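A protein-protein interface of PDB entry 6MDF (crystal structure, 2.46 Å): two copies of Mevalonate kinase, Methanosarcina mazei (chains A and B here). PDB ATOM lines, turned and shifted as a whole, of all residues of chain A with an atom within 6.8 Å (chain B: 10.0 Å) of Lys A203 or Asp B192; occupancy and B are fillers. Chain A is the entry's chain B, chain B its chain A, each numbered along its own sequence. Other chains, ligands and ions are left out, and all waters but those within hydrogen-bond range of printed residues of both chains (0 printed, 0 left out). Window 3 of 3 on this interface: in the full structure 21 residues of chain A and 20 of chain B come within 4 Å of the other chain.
The side-chain carboxylate (OD2) of Asp B192 is in salt-bridge range of the side-chain amino group (NZ) of Lys A203, 3.9 Å away.
Leu B193 touches Ser A200 (CD1 to O, 3.7 Å).
Leu B197 touches Ser A200 (CD2 to OG, 3.6 Å).
CG1 of Ile A204 touches CD1 of Leu B193, 3.6 Å away.
Tyr B190 touches Leu A223 (CZ to CD2, 3.9 Å).
Leu A223 touches Leu B193 (CD2 to CD2, 3.8 Å).
No residue of chain B comes within 4 Å of Gly A202.
Ile A204 touches just one residue of chain B: Leu B193 (3.6 Å).
Gly A208 touches none of the printed residues of chain B.
Ser B189 touches none of the printed residues of chain A.
Of the printed residues of chain A, Tyr B190 touches Leu A223 (3.9 Å).
Asp B192 touches just one residue of chain A: Lys A203 (3.4 Å).
Printed residues of chain A within 4 Å of Leu B193: Ser A200, Ile A204 and Leu A223.
The nearest residue of chain B that does not touch Lys A203 is Leu B193 (4.5 Å).
The nearest printed residue of chain A that does not touch Leu B193 is Ile A207 (4.1 Å).
Printed residues of chain A that touch a printed residue of chain B: Ser A200, Lys A203, Ile A204 and Leu A223.
Hydrophobic or aromatic side chains of chain A within 4 Å of the printed part of chain B: Ile A204 and Leu A223.
Printed residues of chain B that touch a printed residue of chain A: Tyr B190, Asp B192, Leu B193 and Leu B197.
Hydrophobic or aromatic side chains of chain B within 4 Å of the printed part of chain A: Tyr B190, Leu B193 and Leu B197.
Along chain B the printed residues that touch a printed residue of chain A span positions 190 to 197.
Among the printed residues, 6 pairs touch across the chains.
Among the printed residues, Asp or Glu carboxylates within 4 Å of a Lys or Arg side-chain nitrogen of the other chain: Lys A203 with Asp B192 (3.9 Å).
2 positions are printed for both chains.
Of the 6 pairs that touch across the chains among the printed residues, none has its exchanged pair printed and touching as well.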
ATOM      1  N   GLU A  24      29.241 -37.944   0.721  1.00  0.00           N
ATOM      2  CA  GLU A  24      28.219 -37.077   0.159  1.00  0.00           C
ATOM      3  C   GLU A  24      27.961 -37.454  -1.292  1.00  0.00           C
ATOM      4  O   GLU A  24      28.724 -38.197  -1.915  1.00  0.00           O
ATOM      5  CB  GLU A  24      28.621 -35.599   0.260  1.00  0.00           C
ATOM      6  CG  GLU A  24      28.822 -35.103   1.683  1.00  0.00           C
ATOM      7  CD  GLU A  24      27.527 -35.044   2.469  1.00  0.00           C
ATOM      8  OE1 GLU A  24      26.444 -35.123   1.849  1.00  0.00           O
ATOM      9  OE2 GLU A  24      27.592 -34.920   3.712  1.00  0.00           O
ATOM     10  N   THR A  25      26.867 -36.924  -1.828  1.00  0.00           N
ATOM     11  CA  THR A  25      26.451 -37.232  -3.188  1.00  0.00           C
ATOM     12  C   THR A  25      27.134 -36.305  -4.185  1.00  0.00           C
ATOM     13  O   THR A  25      27.489 -35.167  -3.868  1.00  0.00           O
ATOM     14  CB  THR A  25      24.934 -37.112  -3.331  1.00  0.00           C
ATOM     15  OG1 THR A  25      24.302 -37.576  -2.133  1.00  0.00           O
ATOM     16  CG2 THR A  25      24.442 -37.945  -4.503  1.00  0.00           C
ATOM     17  N   MET A 198      30.365 -29.502   3.984  1.00  0.00           N
ATOM     18  CA  MET A 198      30.363 -30.751   3.230  1.00  0.00           C
ATOM     19  C   MET A 198      28.947 -31.276   3.044  1.00  0.00           C
ATOM     20  O   MET A 198      28.609 -31.812   1.982  1.00  0.00           O
ATOM     21  CB  MET A 198      31.227 -31.792   3.939  1.00  0.00           C
ATOM     22  CG  MET A 198      32.668 -31.383   4.113  1.00  0.00           C
ATOM     23  SD  MET A 198      33.506 -31.197   2.533  1.00  0.00           S
ATOM     24  CE  MET A 198      35.021 -30.420   3.078  1.00  0.00           C
ATOM     25  N   THR A 199      28.108 -31.144   4.076  1.00  0.00           N
ATOM     26  CA  THR A 199      26.709 -31.544   3.966  1.00  0.00           C
ATOM     27  C   THR A 199      25.965 -30.677   2.958  1.00  0.00           C
ATOM     28  O   THR A 199      25.123 -31.177   2.201  1.00  0.00           O
ATOM     29  CB  THR A 199      26.038 -31.469   5.340  1.00  0.00           C
ATOM     30  OG1 THR A 199      26.695 -32.365   6.244  1.00  0.00           O
ATOM     31  CG2 THR A 199      24.566 -31.840   5.247  1.00  0.00           C
ATOM     32  N   SER A 200      26.266 -29.376   2.933  1.00  0.00           N
ATOM     33  CA  SER A 200      25.608 -28.481   1.988  1.00  0.00           C
ATOM     34  C   SER A 200      25.933 -28.862   0.551  1.00  0.00           C
ATOM     35  O   SER A 200      25.056 -28.819  -0.320  1.00  0.00           O
ATOM     36  CB  SER A 200      26.014 -27.036   2.263  1.00  0.00           C
ATOM     37  OG  SER A 200      25.661 -26.664   3.579  1.00  0.00           O
ATOM     38  N   ILE A 201      27.188 -29.233   0.284  1.00  0.00           N
ATOM     39  CA  ILE A 201      27.552 -29.682  -1.056  1.00  0.00           C
ATOM     40  C   ILE A 201      26.738 -30.909  -1.437  1.00  0.00           C
ATOM     41  O   ILE A 201      26.200 -30.997  -2.548  1.00  0.00           O
ATOM     42  CB  ILE A 201      29.065 -29.959  -1.144  1.00  0.00           C
ATOM     43  CG1 ILE A 201      29.862 -28.680  -0.886  1.00  0.00           C
ATOM     44  CG2 ILE A 201      29.416 -30.531  -2.501  1.00  0.00           C
ATOM     45  CD1 ILE A 201      31.369 -28.902  -0.832  1.00  0.00           C
ATOM     46  N   GLY A 202      26.628 -31.871  -0.519  1.00  0.00           N
ATOM     47  CA  GLY A 202      25.816 -33.043  -0.792  1.00  0.00           C
ATOM     48  C   GLY A 202      24.357 -32.698  -1.018  1.00  0.00           C
ATOM     49  O   GLY A 202      23.684 -33.319  -1.845  1.00  0.00           O
ATOM     50  N   LYS A 203      23.850 -31.700  -0.288  1.00  0.00           N
ATOM     51  CA  LYS A 203      22.473 -31.264  -0.492  1.00  0.00           C
ATOM     52  C   LYS A 203      22.283 -30.634  -1.868  1.00  0.00           C
ATOM     53  O   LYS A 203      21.218 -30.794  -2.477  1.00  0.00           O
ATOM     54  CB  LYS A 203      22.064 -30.289   0.610  1.00  0.00           C
ATOM     55  CG  LYS A 203      20.602 -29.883   0.556  1.00  0.00           C
ATOM     56  CD  LYS A 203      20.011 -29.731   1.943  1.00  0.00           C
ATOM     57  CE  LYS A 203      18.685 -30.468   2.051  1.00  0.00           C
ATOM     58  NZ  LYS A 203      17.737 -30.052   0.980  1.00  0.00           N
ATOM     59  N   ILE A 204      23.299 -29.927  -2.372  1.00  0.00           N
ATOM     60  CA  ILE A 204      23.241 -29.394  -3.731  1.00  0.00           C
ATOM     61  C   ILE A 204      23.101 -30.527  -4.739  1.00  0.00           C
ATOM     62  O   ILE A 204      22.336 -30.429  -5.705  1.00  0.00           O
ATOM     63  CB  ILE A 204      24.484 -28.534  -4.023  1.00  0.00           C
ATOM     64  CG1 ILE A 204      24.531 -27.325  -3.091  1.00  0.00           C
ATOM     65  CG2 ILE A 204      24.503 -28.082  -5.474  1.00  0.00           C
ATOM     66  CD1 ILE A 204      25.736 -26.446  -3.309  1.00  0.00           C
ATOM     67  N   SER A 205      23.832 -31.622  -4.526  1.00  0.00           N
ATOM     68  CA  SER A 205      23.745 -32.758  -5.436  1.00  0.00           C
ATOM     69  C   SER A 205      22.357 -33.385  -5.411  1.00  0.00           C
ATOM     70  O   SER A 205      21.832 -33.788  -6.455  1.00  0.00           O
ATOM     71  CB  SER A 205      24.806 -33.799  -5.079  1.00  0.00           C
ATOM     72  OG  SER A 205      26.096 -33.218  -5.033  1.00  0.00           O
ATOM     73  N   ARG A 206      21.750 -33.483  -4.225  1.00  0.00           N
ATOM     74  CA  ARG A 206      20.421 -34.076  -4.127  1.00  0.00           C
ATOM     75  C   ARG A 206      19.378 -33.210  -4.823  1.00  0.00           C
ATOM     76  O   ARG A 206      18.519 -33.726  -5.546  1.00  0.00           O
ATOM     77  CB  ARG A 206      20.050 -34.295  -2.661  1.00  0.00           C
ATOM     78  N   ILE A 207      19.437 -31.892  -4.615  1.00  0.00           N
ATOM     79  CA  ILE A 207      18.533 -30.992  -5.326  1.00  0.00           C
ATOM     80  C   ILE A 207      18.812 -31.037  -6.821  1.00  0.00           C
ATOM     81  O   ILE A 207      17.887 -31.088  -7.641  1.00  0.00           O
ATOM     82  CB  ILE A 207      18.654 -29.561  -4.769  1.00  0.00           C
ATOM     83  CG1 ILE A 207      18.362 -29.543  -3.266  1.00  0.00           C
ATOM     84  CG2 ILE A 207      17.718 -28.619  -5.513  1.00  0.00           C
ATOM     85  CD1 ILE A 207      18.591 -28.197  -2.612  1.00  0.00           C
ATOM     86  N   GLY A 208      20.094 -31.036  -7.199  1.00  0.00           N
ATOM     87  CA  GLY A 208      20.446 -31.035  -8.609  1.00  0.00           C
ATOM     88  C   GLY A 208      19.977 -32.270  -9.348  1.00  0.00           C
ATOM     89  O   GLY A 208      19.726 -32.217 -10.555  1.00  0.00           O
ATOM     90  N   LEU A 223      22.656 -23.524  -9.139  1.00  0.00           N
ATOM     91  CA  LEU A 223      23.182 -24.435  -8.127  1.00  0.00           C
ATOM     92  C   LEU A 223      24.669 -24.693  -8.331  1.00  0.00           C
ATOM     93  O   LEU A 223      25.391 -24.951  -7.363  1.00  0.00           O
ATOM     94  CB  LEU A 223      22.420 -25.759  -8.141  1.00  0.00           C
ATOM     95  CG  LEU A 223      21.058 -25.811  -7.451  1.00  0.00           C
ATOM     96  CD1 LEU A 223      20.685 -27.256  -7.158  1.00  0.00           C
ATOM     97  CD2 LEU A 223      21.062 -24.985  -6.180  1.00  0.00           C
ATOM     98  N   LEU B 186      17.067 -16.044  -3.406  1.00  0.00           N
ATOM     99  CA  LEU B 186      17.831 -17.284  -3.449  1.00  0.00           C
ATOM    100  C   LEU B 186      17.541 -18.135  -2.221  1.00  0.00           C
ATOM    101  O   LEU B 186      17.411 -19.359  -2.321  1.00  0.00           O
ATOM    102  CB  LEU B 186      19.320 -16.974  -3.543  1.00  0.00           C
ATOM    103  CG  LEU B 186      20.242 -18.174  -3.268  1.00  0.00           C
ATOM    104  CD1 LEU B 186      20.137 -19.162  -4.404  1.00  0.00           C
ATOM    105  CD2 LEU B 186      21.694 -17.760  -3.018  1.00  0.00           C
ATOM    106  N   ARG B 187      17.445 -17.497  -1.048  1.00  0.00           N
ATOM    107  CA  ARG B 187      17.098 -18.221   0.172  1.00  0.00           C
ATOM    108  C   ARG B 187      15.709 -18.841   0.066  1.00  0.00           C
ATOM    109  O   ARG B 187      15.495 -19.986   0.487  1.00  0.00           O
ATOM    110  CB  ARG B 187      17.182 -17.277   1.374  1.00  0.00           C
ATOM    111  CG  ARG B 187      16.937 -17.931   2.718  1.00  0.00           C
ATOM    112  CD  ARG B 187      17.210 -16.951   3.854  1.00  0.00           C
ATOM    113  NE  ARG B 187      17.044 -17.544   5.181  1.00  0.00           N
ATOM    114  CZ  ARG B 187      15.919 -17.499   5.887  1.00  0.00           C
ATOM    115  NH1 ARG B 187      14.847 -16.894   5.393  1.00  0.00           N
ATOM    116  NH2 ARG B 187      15.863 -18.058   7.088  1.00  0.00           N
ATOM    117  N   GLU B 188      14.755 -18.104  -0.512  1.00  0.00           N
ATOM    118  CA  GLU B 188      13.406 -18.638  -0.670  1.00  0.00           C
ATOM    119  C   GLU B 188      13.365 -19.773  -1.683  1.00  0.00           C
ATOM    120  O   GLU B 188      12.562 -20.701  -1.532  1.00  0.00           O
ATOM    121  CB  GLU B 188      12.436 -17.524  -1.078  1.00  0.00           C
ATOM    122  CG  GLU B 188      12.199 -16.483   0.008  1.00  0.00           C
ATOM    123  CD  GLU B 188      11.456 -15.255  -0.490  1.00  0.00           C
ATOM    124  OE1 GLU B 188      11.427 -15.027  -1.721  1.00  0.00           O
ATOM    125  OE2 GLU B 188      10.903 -14.514   0.352  1.00  0.00           O
ATOM    126  N   SER B 189      14.221 -19.729  -2.709  1.00  0.00           N
ATOM    127  CA  SER B 189      14.200 -20.769  -3.734  1.00  0.00           C
ATOM    128  C   SER B 189      14.665 -22.112  -3.180  1.00  0.00           C
ATOM    129  O   SER B 189      14.094 -23.156  -3.515  1.00  0.00           O
ATOM    130  CB  SER B 189      15.066 -20.355  -4.925  1.00  0.00           C
ATOM    131  OG  SER B 189      14.469 -19.292  -5.648  1.00  0.00           O
ATOM    132  N   TYR B 190      15.699 -22.107  -2.339  1.00  0.00           N
ATOM    133  CA  TYR B 190      16.266 -23.327  -1.764  1.00  0.00           C
ATOM    134  C   TYR B 190      16.453 -23.108  -0.271  1.00  0.00           C
ATOM    135  O   TYR B 190      17.562 -22.809   0.192  1.00  0.00           O
ATOM    136  CB  TYR B 190      17.590 -23.697  -2.437  1.00  0.00           C
ATOM    137  CG  TYR B 190      17.562 -23.605  -3.945  1.00  0.00           C
ATOM    138  CD1 TYR B 190      17.117 -24.672  -4.714  1.00  0.00           C
ATOM    139  CD2 TYR B 190      17.982 -22.453  -4.598  1.00  0.00           C
ATOM    140  CE1 TYR B 190      17.088 -24.596  -6.096  1.00  0.00           C
ATOM    141  CE2 TYR B 190      17.958 -22.365  -5.981  1.00  0.00           C
ATOM    142  CZ  TYR B 190      17.510 -23.442  -6.726  1.00  0.00           C
ATOM    143  OH  TYR B 190      17.481 -23.367  -8.100  1.00  0.00           O
ATOM    144  N   PRO B 191      15.384 -23.243   0.517  1.00  0.00           N
ATOM    145  CA  PRO B 191      15.507 -22.940   1.954  1.00  0.00           C
ATOM    146  C   PRO B 191      16.433 -23.891   2.693  1.00  0.00           C
ATOM    147  O   PRO B 191      17.307 -23.439   3.444  1.00  0.00           O
ATOM    148  CB  PRO B 191      14.056 -23.031   2.452  1.00  0.00           C
ATOM    149  CG  PRO B 191      13.211 -22.875   1.222  1.00  0.00           C
ATOM    150  CD  PRO B 191      13.993 -23.524   0.127  1.00  0.00           C
ATOM    151  N   ASP B 192      16.275 -25.201   2.493  1.00  0.00           N
ATOM    152  CA  ASP B 192      17.113 -26.174   3.183  1.00  0.00           C
ATOM    153  C   ASP B 192      18.570 -26.109   2.750  1.00  0.00           C
ATOM    154  O   ASP B 192      19.417 -26.738   3.394  1.00  0.00           O
ATOM    155  CB  ASP B 192      16.579 -27.588   2.957  1.00  0.00           C
ATOM    156  CG  ASP B 192      15.068 -27.643   2.925  1.00  0.00           C
ATOM    157  OD1 ASP B 192      14.436 -27.290   3.944  1.00  0.00           O
ATOM    158  OD2 ASP B 192      14.513 -28.046   1.879  1.00  0.00           O
ATOM    159  N   LEU B 193      18.881 -25.376   1.686  1.00  0.00           N
ATOM    160  CA  LEU B 193      20.256 -25.211   1.240  1.00  0.00           C
ATOM    161  C   LEU B 193      20.866 -23.899   1.717  1.00  0.00           C
ATOM    162  O   LEU B 193      21.982 -23.892   2.246  1.00  0.00           O
ATOM    163  CB  LEU B 193      20.320 -25.298  -0.288  1.00  0.00           C
ATOM    164  CG  LEU B 193      21.665 -24.981  -0.935  1.00  0.00           C
ATOM    165  CD1 LEU B 193      22.749 -25.881  -0.363  1.00  0.00           C
ATOM    166  CD2 LEU B 193      21.571 -25.132  -2.444  1.00  0.00           C
ATOM    167  N   ILE B 194      20.147 -22.789   1.556  1.00  0.00           N
ATOM    168  CA  ILE B 194      20.726 -21.480   1.844  1.00  0.00           C
ATOM    169  C   ILE B 194      20.702 -21.180   3.338  1.00  0.00           C
ATOM    170  O   ILE B 194      21.658 -20.615   3.879  1.00  0.00           O
ATOM    171  CB  ILE B 194      19.997 -20.394   1.034  1.00  0.00           C
ATOM    172  CG1 ILE B 194      20.121 -20.684  -0.465  1.00  0.00           C
ATOM    173  CG2 ILE B 194      20.547 -19.013   1.375  1.00  0.00           C
ATOM    174  CD1 ILE B 194      21.553 -20.833  -0.947  1.00  0.00           C
ATOM    175  N   GLU B 195      19.617 -21.538   4.025  1.00  0.00           N
ATOM    176  CA  GLU B 195      19.531 -21.252   5.456  1.00  0.00           C
ATOM    177  C   GLU B 195      20.665 -21.881   6.260  1.00  0.00           C
ATOM    178  O   GLU B 195      21.229 -21.182   7.120  1.00  0.00           O
ATOM    179  CB  GLU B 195      18.161 -21.685   5.996  1.00  0.00           C
ATOM    180  N   PRO B 196      21.054 -23.146   6.049  1.00  0.00           N
ATOM    181  CA  PRO B 196      22.264 -23.647   6.724  1.00  0.00           C
ATOM    182  C   PRO B 196      23.518 -22.857   6.393  1.00  0.00           C
ATOM    183  O   PRO B 196      24.406 -22.743   7.248  1.00  0.00           O
ATOM    184  CB  PRO B 196      22.369 -25.095   6.228  1.00  0.00           C
ATOM    185  CG  PRO B 196      20.984 -25.468   5.876  1.00  0.00           C
ATOM    186  CD  PRO B 196      20.354 -24.223   5.325  1.00  0.00           C
ATOM    187  N   LEU B 197      23.630 -22.319   5.174  1.00  0.00           N
ATOM    188  CA  LEU B 197      24.782 -21.482   4.850  1.00  0.00           C
ATOM    189  C   LEU B 197      24.795 -20.216   5.694  1.00  0.00           C
ATOM    190  O   LEU B 197      25.871 -19.709   6.032  1.00  0.00           O
ATOM    191  CB  LEU B 197      24.787 -21.128   3.362  1.00  0.00           C
ATOM    192  CG  LEU B 197      24.890 -22.287   2.366  1.00  0.00           C
ATOM    193  CD1 LEU B 197      24.992 -21.765   0.940  1.00  0.00           C
ATOM    194  CD2 LEU B 197      26.072 -23.175   2.699  1.00  0.00           C
ATOM    195  N   MET B 198      23.616 -19.697   6.045  1.00  0.00           N
ATOM    196  CA  MET B 198      23.544 -18.568   6.965  1.00  0.00           C
ATOM    197  C   MET B 198      24.009 -18.965   8.360  1.00  0.00           C
ATOM    198  O   MET B 198      24.645 -18.169   9.059  1.00  0.00           O
ATOM    199  CB  MET B 198      22.117 -18.025   7.014  1.00  0.00           C
ATOM    200  CG  MET B 198      21.582 -17.570   5.672  1.00  0.00           C
ATOM    201  SD  MET B 198      22.419 -16.097   5.064  1.00  0.00           S
ATOM    202  CE  MET B 198      21.594 -15.885   3.488  1.00  0.00           C
ATOM    203  N   THR B 199      23.692 -20.192   8.783  1.00  0.00           N
ATOM    204  CA  THR B 199      24.186 -20.685  10.064  1.00  0.00           C
ATOM    205  C   THR B 199      25.706 -20.795  10.059  1.00  0.00           C
ATOM    206  O   THR B 199      26.359 -20.525  11.073  1.00  0.00           O
ATOM    207  CB  THR B 199      23.553 -22.040  10.387  1.00  0.00           C
ATOM    208  OG1 THR B 199      22.128 -21.942  10.291  1.00  0.00           O
ATOM    209  CG2 THR B 199      23.929 -22.486  11.791  1.00  0.00           C
